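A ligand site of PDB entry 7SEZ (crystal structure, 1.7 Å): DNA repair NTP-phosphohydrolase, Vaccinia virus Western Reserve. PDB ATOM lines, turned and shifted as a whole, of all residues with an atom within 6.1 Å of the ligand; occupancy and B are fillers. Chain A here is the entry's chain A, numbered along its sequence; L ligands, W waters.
CZ of Phe 35 touches O10 of the ligand, at 3.7 Å.
CE2 of Phe 54 touches N5 of the ligand, 3.4 Å away.
Gln 57 touches the ligand (NE2 to C7, 3.5 Å).
Lys 112 touches the ligand.
CD2 of Phe 154 touches O11 of the ligand, 3.7 Å away.
Ile 159 touches the ligand (O to O9, 3.99 Å).
Hydrophobic or aromatic side chains within 4 Å of the ligand: His 33, Phe 35, Phe 54, Phe 154 and Tyr 158.
Within 4 Å of the ligand: Glu 16, His 33, Phe 35, Arg 50, Phe 54, Gln 57, Lys 112, Asp 151, Phe 154, Tyr 158 and Ile 159.
The nearest printed residue that does not touch the ligand is Thr 149 (4.05 Å).
The guanidinium group (NH2) of Arg 50 lies within hydrogen-bond range of the side-chain amide oxygen (OE1) of Gln 57 (2.8 Å).
OD1 of Asp 151 is in hydrogen-bond range of N of Phe 154 (2.9 Å).
N of Tyr 158 is in hydrogen-bond range of O of Thr 149 (2.8 Å).
OH of Tyr 158 lies within hydrogen-bond range of O11 of the ligand (3.3 Å).
O5 of the ligand lies within salt-bridge range of NH2 of Arg 50, 3.2 Å away.
O2 of the ligand lies close to NE2 of His 33 (2.9 Å).
The side-chain carboxylate (OE2) of Glu 16 is in hydrogen-bond range of a nitrogen (N4) of the ligand, 2.7 Å away.
The side-chain carboxylate (OD2) of Asp 151 lies within hydrogen-bond range of a nitrogen (N3) of the ligand.
Water W3 bridges an oxygen (O5) of the ligand and the guanidinium group (NE) of Arg 50.
Water W6 bridges O of Phe 54 and O11 of the ligand.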
ATOM      1  N   ARG A  15     -14.272  -4.050   2.625  1.00  0.00           N
ATOM      2  CA  ARG A  15     -15.417  -3.238   2.197  1.00  0.00           C
ATOM      3  C   ARG A  15     -15.061  -1.962   1.460  1.00  0.00           C
ATOM      4  O   ARG A  15     -15.904  -1.417   0.747  1.00  0.00           O
ATOM      5  CB  ARG A  15     -16.291  -2.853   3.402  1.00  0.00           C
ATOM      6  CG  ARG A  15     -16.999  -4.008   4.011  1.00  0.00           C
ATOM      7  CD  ARG A  15     -18.327  -3.502   4.509  1.00  0.00           C
ATOM      8  NE  ARG A  15     -18.134  -2.704   5.701  1.00  0.00           N
ATOM      9  CZ  ARG A  15     -19.040  -1.887   6.217  1.00  0.00           C
ATOM     10  NH1 ARG A  15     -20.218  -1.715   5.593  1.00  0.00           N
ATOM     11  NH2 ARG A  15     -18.766  -1.249   7.350  1.00  0.00           N
ATOM     12  N   GLU A  16     -13.851  -1.459   1.671  1.00  0.00           N
ATOM     13  CA  GLU A  16     -13.475  -0.130   1.186  1.00  0.00           C
ATOM     14  C   GLU A  16     -12.107  -0.095   0.537  1.00  0.00           C
ATOM     15  O   GLU A  16     -11.183  -0.829   0.931  1.00  0.00           O
ATOM     16  CB  GLU A  16     -13.483   0.906   2.320  1.00  0.00           C
ATOM     17  CG  GLU A  16     -14.857   1.127   2.935  1.00  0.00           C
ATOM     18  CD  GLU A  16     -14.821   2.070   4.140  1.00  0.00           C
ATOM     19  OE1 GLU A  16     -14.075   1.804   5.111  1.00  0.00           O
ATOM     20  OE2 GLU A  16     -15.534   3.097   4.090  1.00  0.00           O
ATOM     21  N   HIS A  33     -17.895  17.627   2.502  1.00  0.00           N
ATOM     22  CA  HIS A  33     -17.835  16.920   3.775  1.00  0.00           C
ATOM     23  C   HIS A  33     -16.504  17.111   4.479  1.00  0.00           C
ATOM     24  O   HIS A  33     -15.447  16.824   3.928  1.00  0.00           O
ATOM     25  CB  HIS A  33     -18.075  15.428   3.570  1.00  0.00           C
ATOM     26  CG  HIS A  33     -19.527  15.060   3.564  1.00  0.00           C
ATOM     27  ND1 HIS A  33     -20.336  15.233   2.469  1.00  0.00           N
ATOM     28  CD2 HIS A  33     -20.311  14.556   4.548  1.00  0.00           C
ATOM     29  CE1 HIS A  33     -21.567  14.847   2.767  1.00  0.00           C
ATOM     30  NE2 HIS A  33     -21.581  14.426   4.018  1.00  0.00           N
ATOM     31  N   PHE A  35     -14.279  16.281   7.965  1.00  0.00           N
ATOM     32  CA  PHE A  35     -14.080  15.375   9.083  1.00  0.00           C
ATOM     33  C   PHE A  35     -13.082  15.953  10.082  1.00  0.00           C
ATOM     34  O   PHE A  35     -12.041  16.542   9.708  1.00  0.00           O
ATOM     35  CB  PHE A  35     -13.534  14.021   8.623  1.00  0.00           C
ATOM     36  CG  PHE A  35     -14.444  13.240   7.739  1.00  0.00           C
ATOM     37  CD1 PHE A  35     -15.483  12.518   8.283  1.00  0.00           C
ATOM     38  CD2 PHE A  35     -14.172  13.128   6.390  1.00  0.00           C
ATOM     39  CE1 PHE A  35     -16.295  11.748   7.469  1.00  0.00           C
ATOM     40  CE2 PHE A  35     -14.975  12.355   5.568  1.00  0.00           C
ATOM     41  CZ  PHE A  35     -16.040  11.659   6.105  1.00  0.00           C
ATOM     42  N   ARG A  50     -21.144   5.073  14.126  1.00  0.00           N
ATOM     43  CA  ARG A  50     -22.310   5.636  13.472  1.00  0.00           C
ATOM     44  C   ARG A  50     -23.589   5.026  14.047  1.00  0.00           C
ATOM     45  O   ARG A  50     -23.639   3.839  14.320  1.00  0.00           O
ATOM     46  CB  ARG A  50     -22.223   5.394  11.967  1.00  0.00           C
ATOM     47  CG  ARG A  50     -23.098   6.304  11.120  1.00  0.00           C
ATOM     48  CD  ARG A  50     -22.854   5.928   9.652  1.00  0.00           C
ATOM     49  NE  ARG A  50     -23.423   6.856   8.670  1.00  0.00           N
ATOM     50  CZ  ARG A  50     -24.481   6.591   7.913  1.00  0.00           C
ATOM     51  NH1 ARG A  50     -25.138   5.446   8.045  1.00  0.00           N
ATOM     52  NH2 ARG A  50     -24.894   7.489   7.017  1.00  0.00           N
ATOM     53  N   PHE A  54     -23.888   1.622   7.582  1.00  0.00           N
ATOM     54  CA  PHE A  54     -24.003   1.812   6.120  1.00  0.00           C
ATOM     55  C   PHE A  54     -24.860   0.721   5.481  1.00  0.00           C
ATOM     56  O   PHE A  54     -25.730   0.978   4.615  1.00  0.00           O
ATOM     57  CB  PHE A  54     -22.642   1.818   5.442  1.00  0.00           C
ATOM     58  CG  PHE A  54     -21.746   2.934   5.876  1.00  0.00           C
ATOM     59  CD1 PHE A  54     -22.267   4.161   6.225  1.00  0.00           C
ATOM     60  CD2 PHE A  54     -20.379   2.748   5.912  1.00  0.00           C
ATOM     61  CE1 PHE A  54     -21.426   5.201   6.627  1.00  0.00           C
ATOM     62  CE2 PHE A  54     -19.528   3.785   6.304  1.00  0.00           C
ATOM     63  CZ  PHE A  54     -20.066   4.997   6.682  1.00  0.00           C
ATOM     64  N   ALA A  55     -24.611  -0.517   5.898  1.00  0.00           N
ATOM     65  CA  ALA A  55     -25.351  -1.663   5.365  1.00  0.00           C
ATOM     66  C   ALA A  55     -26.862  -1.567   5.613  1.00  0.00           C
ATOM     67  O   ALA A  55     -27.653  -1.779   4.688  1.00  0.00           O
ATOM     68  CB  ALA A  55     -24.767  -2.981   5.951  1.00  0.00           C
ATOM     69  N   GLN A  57     -28.599   1.176   6.297  1.00  0.00           N
ATOM     70  CA  GLN A  57     -29.064   2.330   5.511  1.00  0.00           C
ATOM     71  C   GLN A  57     -29.375   1.927   4.069  1.00  0.00           C
ATOM     72  O   GLN A  57     -30.448   2.256   3.504  1.00  0.00           O
ATOM     73  CB  GLN A  57     -28.005   3.435   5.533  1.00  0.00           C
ATOM     74  CG  GLN A  57     -28.370   4.585   4.621  1.00  0.00           C
ATOM     75  CD  GLN A  57     -27.490   5.801   4.829  1.00  0.00           C
ATOM     76  OE1 GLN A  57     -27.002   6.061   5.922  1.00  0.00           O
ATOM     77  NE2 GLN A  57     -27.289   6.550   3.752  1.00  0.00           N
ATOM     78  N   ALA A  58     -28.446   1.181   3.477  1.00  0.00           N
ATOM     79  CA  ALA A  58     -28.580   0.742   2.101  1.00  0.00           C
ATOM     80  C   ALA A  58     -29.762  -0.218   1.945  1.00  0.00           C
ATOM     81  O   ALA A  58     -30.577  -0.095   1.014  1.00  0.00           O
ATOM     82  CB  ALA A  58     -27.293   0.083   1.646  1.00  0.00           C
ATOM     83  N   ILE A 107     -16.541   5.818  12.207  1.00  0.00           N
ATOM     84  CA  ILE A 107     -16.429   6.992  11.347  1.00  0.00           C
ATOM     85  C   ILE A 107     -15.734   8.126  12.084  1.00  0.00           C
ATOM     86  O   ILE A 107     -15.836   8.260  13.308  1.00  0.00           O
ATOM     87  CB  ILE A 107     -17.789   7.523  10.870  1.00  0.00           C
ATOM     88  CG1 ILE A 107     -18.728   7.764  12.055  1.00  0.00           C
ATOM     89  CG2 ILE A 107     -18.421   6.572   9.844  1.00  0.00           C
ATOM     90  CD1 ILE A 107     -20.052   8.436  11.685  1.00  0.00           C
ATOM     91  N   LYS A 112     -21.448  18.010   6.849  1.00  0.00           N
ATOM     92  CA  LYS A 112     -21.475  18.789   5.608  1.00  0.00           C
ATOM     93  C   LYS A 112     -21.225  20.279   5.803  1.00  0.00           C
ATOM     94  O   LYS A 112     -21.668  20.873   6.790  1.00  0.00           O
ATOM     95  CB  LYS A 112     -22.813  18.587   4.900  1.00  0.00           C
ATOM     96  CG  LYS A 112     -23.066  17.136   4.536  1.00  0.00           C
ATOM     97  CD  LYS A 112     -24.413  16.883   3.868  1.00  0.00           C
ATOM     98  CE  LYS A 112     -24.798  15.407   3.997  1.00  0.00           C
ATOM     99  NZ  LYS A 112     -25.845  14.979   3.029  1.00  0.00           N
ATOM    100  N   THR A 149     -13.109   7.611  -1.030  1.00  0.00           N
ATOM    101  CA  THR A 149     -13.468   6.246  -0.654  1.00  0.00           C
ATOM    102  C   THR A 149     -14.341   5.531  -1.683  1.00  0.00           C
ATOM    103  O   THR A 149     -15.382   6.034  -2.069  1.00  0.00           O
ATOM    104  CB  THR A 149     -14.196   6.228   0.693  1.00  0.00           C
ATOM    105  OG1 THR A 149     -13.375   6.837   1.693  1.00  0.00           O
ATOM    106  CG2 THR A 149     -14.524   4.777   1.113  1.00  0.00           C
ATOM    107  N   ARG A 150     -13.929   4.356  -2.117  1.00  0.00           N
ATOM    108  CA  ARG A 150     -14.815   3.512  -2.908  1.00  0.00           C
ATOM    109  C   ARG A 150     -15.380   2.417  -2.012  1.00  0.00           C
ATOM    110  O   ARG A 150     -14.635   1.671  -1.367  1.00  0.00           O
ATOM    111  CB  ARG A 150     -14.079   2.871  -4.097  1.00  0.00           C
ATOM    112  CG  ARG A 150     -14.927   1.799  -4.786  1.00  0.00           C
ATOM    113  CD  ARG A 150     -14.281   1.306  -6.073  1.00  0.00           C
ATOM    114  NE  ARG A 150     -14.365   2.302  -7.130  1.00  0.00           N
ATOM    115  CZ  ARG A 150     -15.436   2.489  -7.900  1.00  0.00           C
ATOM    116  NH1 ARG A 150     -16.524   1.725  -7.721  1.00  0.00           N
ATOM    117  NH2 ARG A 150     -15.428   3.418  -8.842  1.00  0.00           N
ATOM    118  N   ASP A 151     -16.695   2.341  -1.951  1.00  0.00           N
ATOM    119  CA  ASP A 151     -17.339   1.261  -1.244  1.00  0.00           C
ATOM    120  C   ASP A 151     -17.453   0.095  -2.195  1.00  0.00           C
ATOM    121  O   ASP A 151     -18.096   0.186  -3.250  1.00  0.00           O
ATOM    122  CB  ASP A 151     -18.723   1.694  -0.706  1.00  0.00           C
ATOM    123  CG  ASP A 151     -19.391   0.593   0.113  1.00  0.00           C
ATOM    124  OD1 ASP A 151     -19.608  -0.509  -0.412  1.00  0.00           O
ATOM    125  OD2 ASP A 151     -19.678   0.832   1.313  1.00  0.00           O
ATOM    126  N   PHE A 154     -21.233  -1.576  -2.565  1.00  0.00           N
ATOM    127  CA  PHE A 154     -22.307  -0.793  -3.175  1.00  0.00           C
ATOM    128  C   PHE A 154     -21.860  -0.057  -4.440  1.00  0.00           C
ATOM    129  O   PHE A 154     -22.682   0.572  -5.106  1.00  0.00           O
ATOM    130  CB  PHE A 154     -22.861   0.198  -2.160  1.00  0.00           C
ATOM    131  CG  PHE A 154     -23.399  -0.457  -0.916  1.00  0.00           C
ATOM    132  CD1 PHE A 154     -24.206  -1.576  -1.003  1.00  0.00           C
ATOM    133  CD2 PHE A 154     -23.049   0.026   0.335  1.00  0.00           C
ATOM    134  CE1 PHE A 154     -24.693  -2.188   0.141  1.00  0.00           C
ATOM    135  CE2 PHE A 154     -23.537  -0.577   1.485  1.00  0.00           C
ATOM    136  CZ  PHE A 154     -24.354  -1.686   1.384  1.00  0.00           C
ATOM    137  N   TYR A 158     -17.068   8.268  -2.499  1.00  0.00           N
ATOM    138  CA  TYR A 158     -17.311   9.405  -1.628  1.00  0.00           C
ATOM    139  C   TYR A 158     -16.064  10.254  -1.468  1.00  0.00           C
ATOM    140  O   TYR A 158     -14.948   9.739  -1.451  1.00  0.00           O
ATOM    141  CB  TYR A 158     -17.776   8.934  -0.239  1.00  0.00           C
ATOM    142  CG  TYR A 158     -18.953   7.999  -0.269  1.00  0.00           C
ATOM    143  CD1 TYR A 158     -18.785   6.631  -0.415  1.00  0.00           C
ATOM    144  CD2 TYR A 158     -20.246   8.488  -0.159  1.00  0.00           C
ATOM    145  CE1 TYR A 158     -19.881   5.782  -0.463  1.00  0.00           C
ATOM    146  CE2 TYR A 158     -21.333   7.660  -0.183  1.00  0.00           C
ATOM    147  CZ  TYR A 158     -21.163   6.309  -0.332  1.00  0.00           C
ATOM    148  OH  TYR A 158     -22.273   5.517  -0.372  1.00  0.00           O
ATOM    149  N   ILE A 159     -16.227  11.568  -1.351  1.00  0.00           N
ATOM    150  CA  ILE A 159     -15.101  12.472  -1.128  1.00  0.00           C
ATOM    151  C   ILE A 159     -15.313  13.226   0.175  1.00  0.00           C
ATOM    152  O   ILE A 159     -16.427  13.684   0.438  1.00  0.00           O
ATOM    153  CB  ILE A 159     -14.949  13.485  -2.288  1.00  0.00           C
ATOM    154  CG1 ILE A 159     -14.821  12.767  -3.621  1.00  0.00           C
ATOM    155  CG2 ILE A 159     -13.753  14.400  -2.047  1.00  0.00           C
ATOM    156  CD1 ILE A 159     -13.528  12.085  -3.802  1.00  0.00           C
ATOM    157  N   GLY A 160     -14.274  13.349   0.982  1.00  0.00           N
ATOM    158  CA  GLY A 160     -14.319  14.203   2.162  1.00  0.00           C
ATOM    159  C   GLY A 160     -12.949  14.773   2.471  1.00  0.00           C
ATOM    160  O   GLY A 160     -11.967  14.368   1.869  1.00  0.00           O
ATOM    161  N   GLU A 183     -27.047  10.725  14.911  1.00  0.00           N
ATOM    162  CA  GLU A 183     -25.897  10.499  14.019  1.00  0.00           C
ATOM    163  C   GLU A 183     -24.905   9.459  14.565  1.00  0.00           C
ATOM    164  O   GLU A 183     -24.301   8.709  13.779  1.00  0.00           O
ATOM    165  CB  GLU A 183     -25.148  11.819  13.785  1.00  0.00           C
ATOM    166  CG  GLU A 183     -25.980  12.874  13.074  1.00  0.00           C
ATOM    167  CD  GLU A 183     -26.383  12.452  11.678  1.00  0.00           C
ATOM    168  OE1 GLU A 183     -25.600  11.725  11.015  1.00  0.00           O
ATOM    169  OE2 GLU A 183     -27.473  12.849  11.232  1.00  0.00           O
ATOM    170  N   LYS A 198     -11.390  -1.022   9.626  1.00  0.00           N
ATOM    171  CA  LYS A 198     -10.964   0.331   9.294  1.00  0.00           C
ATOM    172  C   LYS A 198      -9.784   0.849  10.128  1.00  0.00           C
ATOM    173  O   LYS A 198      -9.302   1.966   9.910  1.00  0.00           O
ATOM    174  CB  LYS A 198     -12.128   1.321   9.475  1.00  0.00           C
ATOM    175  CG  LYS A 198     -13.416   0.929   8.749  1.00  0.00           C
ATOM    176  CD  LYS A 198     -14.475   2.007   8.883  1.00  0.00           C
ATOM    177  CE  LYS A 198     -15.782   1.608   8.193  1.00  0.00           C
ATOM    178  NZ  LYS A 198     -16.862   2.632   8.399  1.00  0.00           N
HETATM  179  P1  LIG L   1     -22.996  11.122   3.235  1.00  0.00           P
HETATM  180  O1  LIG L   1     -23.674  10.144   2.277  1.00  0.00           O
HETATM  181  O2  LIG L   1     -22.367  12.205   2.414  1.00  0.00           O
HETATM  182  O3  LIG L   1     -24.093  11.712   4.261  1.00  0.00           O
HETATM  183  O4  LIG L   1     -21.895  10.372   4.090  1.00  0.00           O
HETATM  184  P2  LIG L   1     -24.819  10.723   5.245  1.00  0.00           P
HETATM  185  O5  LIG L   1     -23.903  10.425   6.415  1.00  0.00           O
HETATM  186  O6  LIG L   1     -26.071  11.355   5.770  1.00  0.00           O
HETATM  187  O7  LIG L   1     -25.161   9.462   4.488  1.00  0.00           O
HETATM  188  C1  LIG L   1     -20.807  11.069   4.681  1.00  0.00           C
HETATM  189  C2  LIG L   1     -19.705  10.224   4.705  1.00  0.00           C
HETATM  190  O8  LIG L   1     -20.081   8.855   5.204  1.00  0.00           O
HETATM  191  C3  LIG L   1     -19.197   9.953   3.208  1.00  0.00           C
HETATM  192  O9  LIG L   1     -18.218  10.989   2.767  1.00  0.00           O
HETATM  193  C4  LIG L   1     -18.647   8.847   3.281  1.00  0.00           C
HETATM  194  O10 LIG L   1     -17.320   8.969   3.909  1.00  0.00           O
HETATM  195  C5  LIG L   1     -19.512   7.984   4.380  1.00  0.00           C
HETATM  196  N1  LIG L   1     -20.468   7.150   3.854  1.00  0.00           N
HETATM  197  C6  LIG L   1     -21.903   7.394   3.766  1.00  0.00           C
HETATM  198  N2  LIG L   1     -22.515   6.166   3.186  1.00  0.00           N
HETATM  199  C7  LIG L   1     -23.927   5.980   2.920  1.00  0.00           C
HETATM  200  C8  LIG L   1     -21.469   5.259   2.976  1.00  0.00           C
HETATM  201  C9  LIG L   1     -21.489   3.844   2.456  1.00  0.00           C
HETATM  202  O11 LIG L   1     -22.503   3.281   2.083  1.00  0.00           O
HETATM  203  N3  LIG L   1     -20.264   3.156   2.343  1.00  0.00           N
HETATM  204  C10 LIG L   1     -19.048   3.766   2.770  1.00  0.00           C
HETATM  205  N4  LIG L   1     -17.847   3.058   2.659  1.00  0.00           N
HETATM  206  N5  LIG L   1     -19.025   5.110   3.265  1.00  0.00           N
HETATM  207  C11 LIG L   1     -20.265   5.831   3.382  1.00  0.00           C
HETATM  208  O   HOH W   1     -17.624   8.919   7.162  1.00  0.00           O
HETATM  209  O   HOH W   2     -15.412   8.609   5.641  1.00  0.00           O
HETATM  210  O   HOH W   3     -22.288   9.534   8.643  1.00  0.00           O
HETATM  211  O   HOH W   4     -19.799  10.323   8.267  1.00  0.00           O
HETATM  212  O   HOH W   5     -24.698   6.673  -0.397  1.00  0.00           O
HETATM  213  O   HOH W   6     -25.319   3.135   2.940  1.00  0.00           O
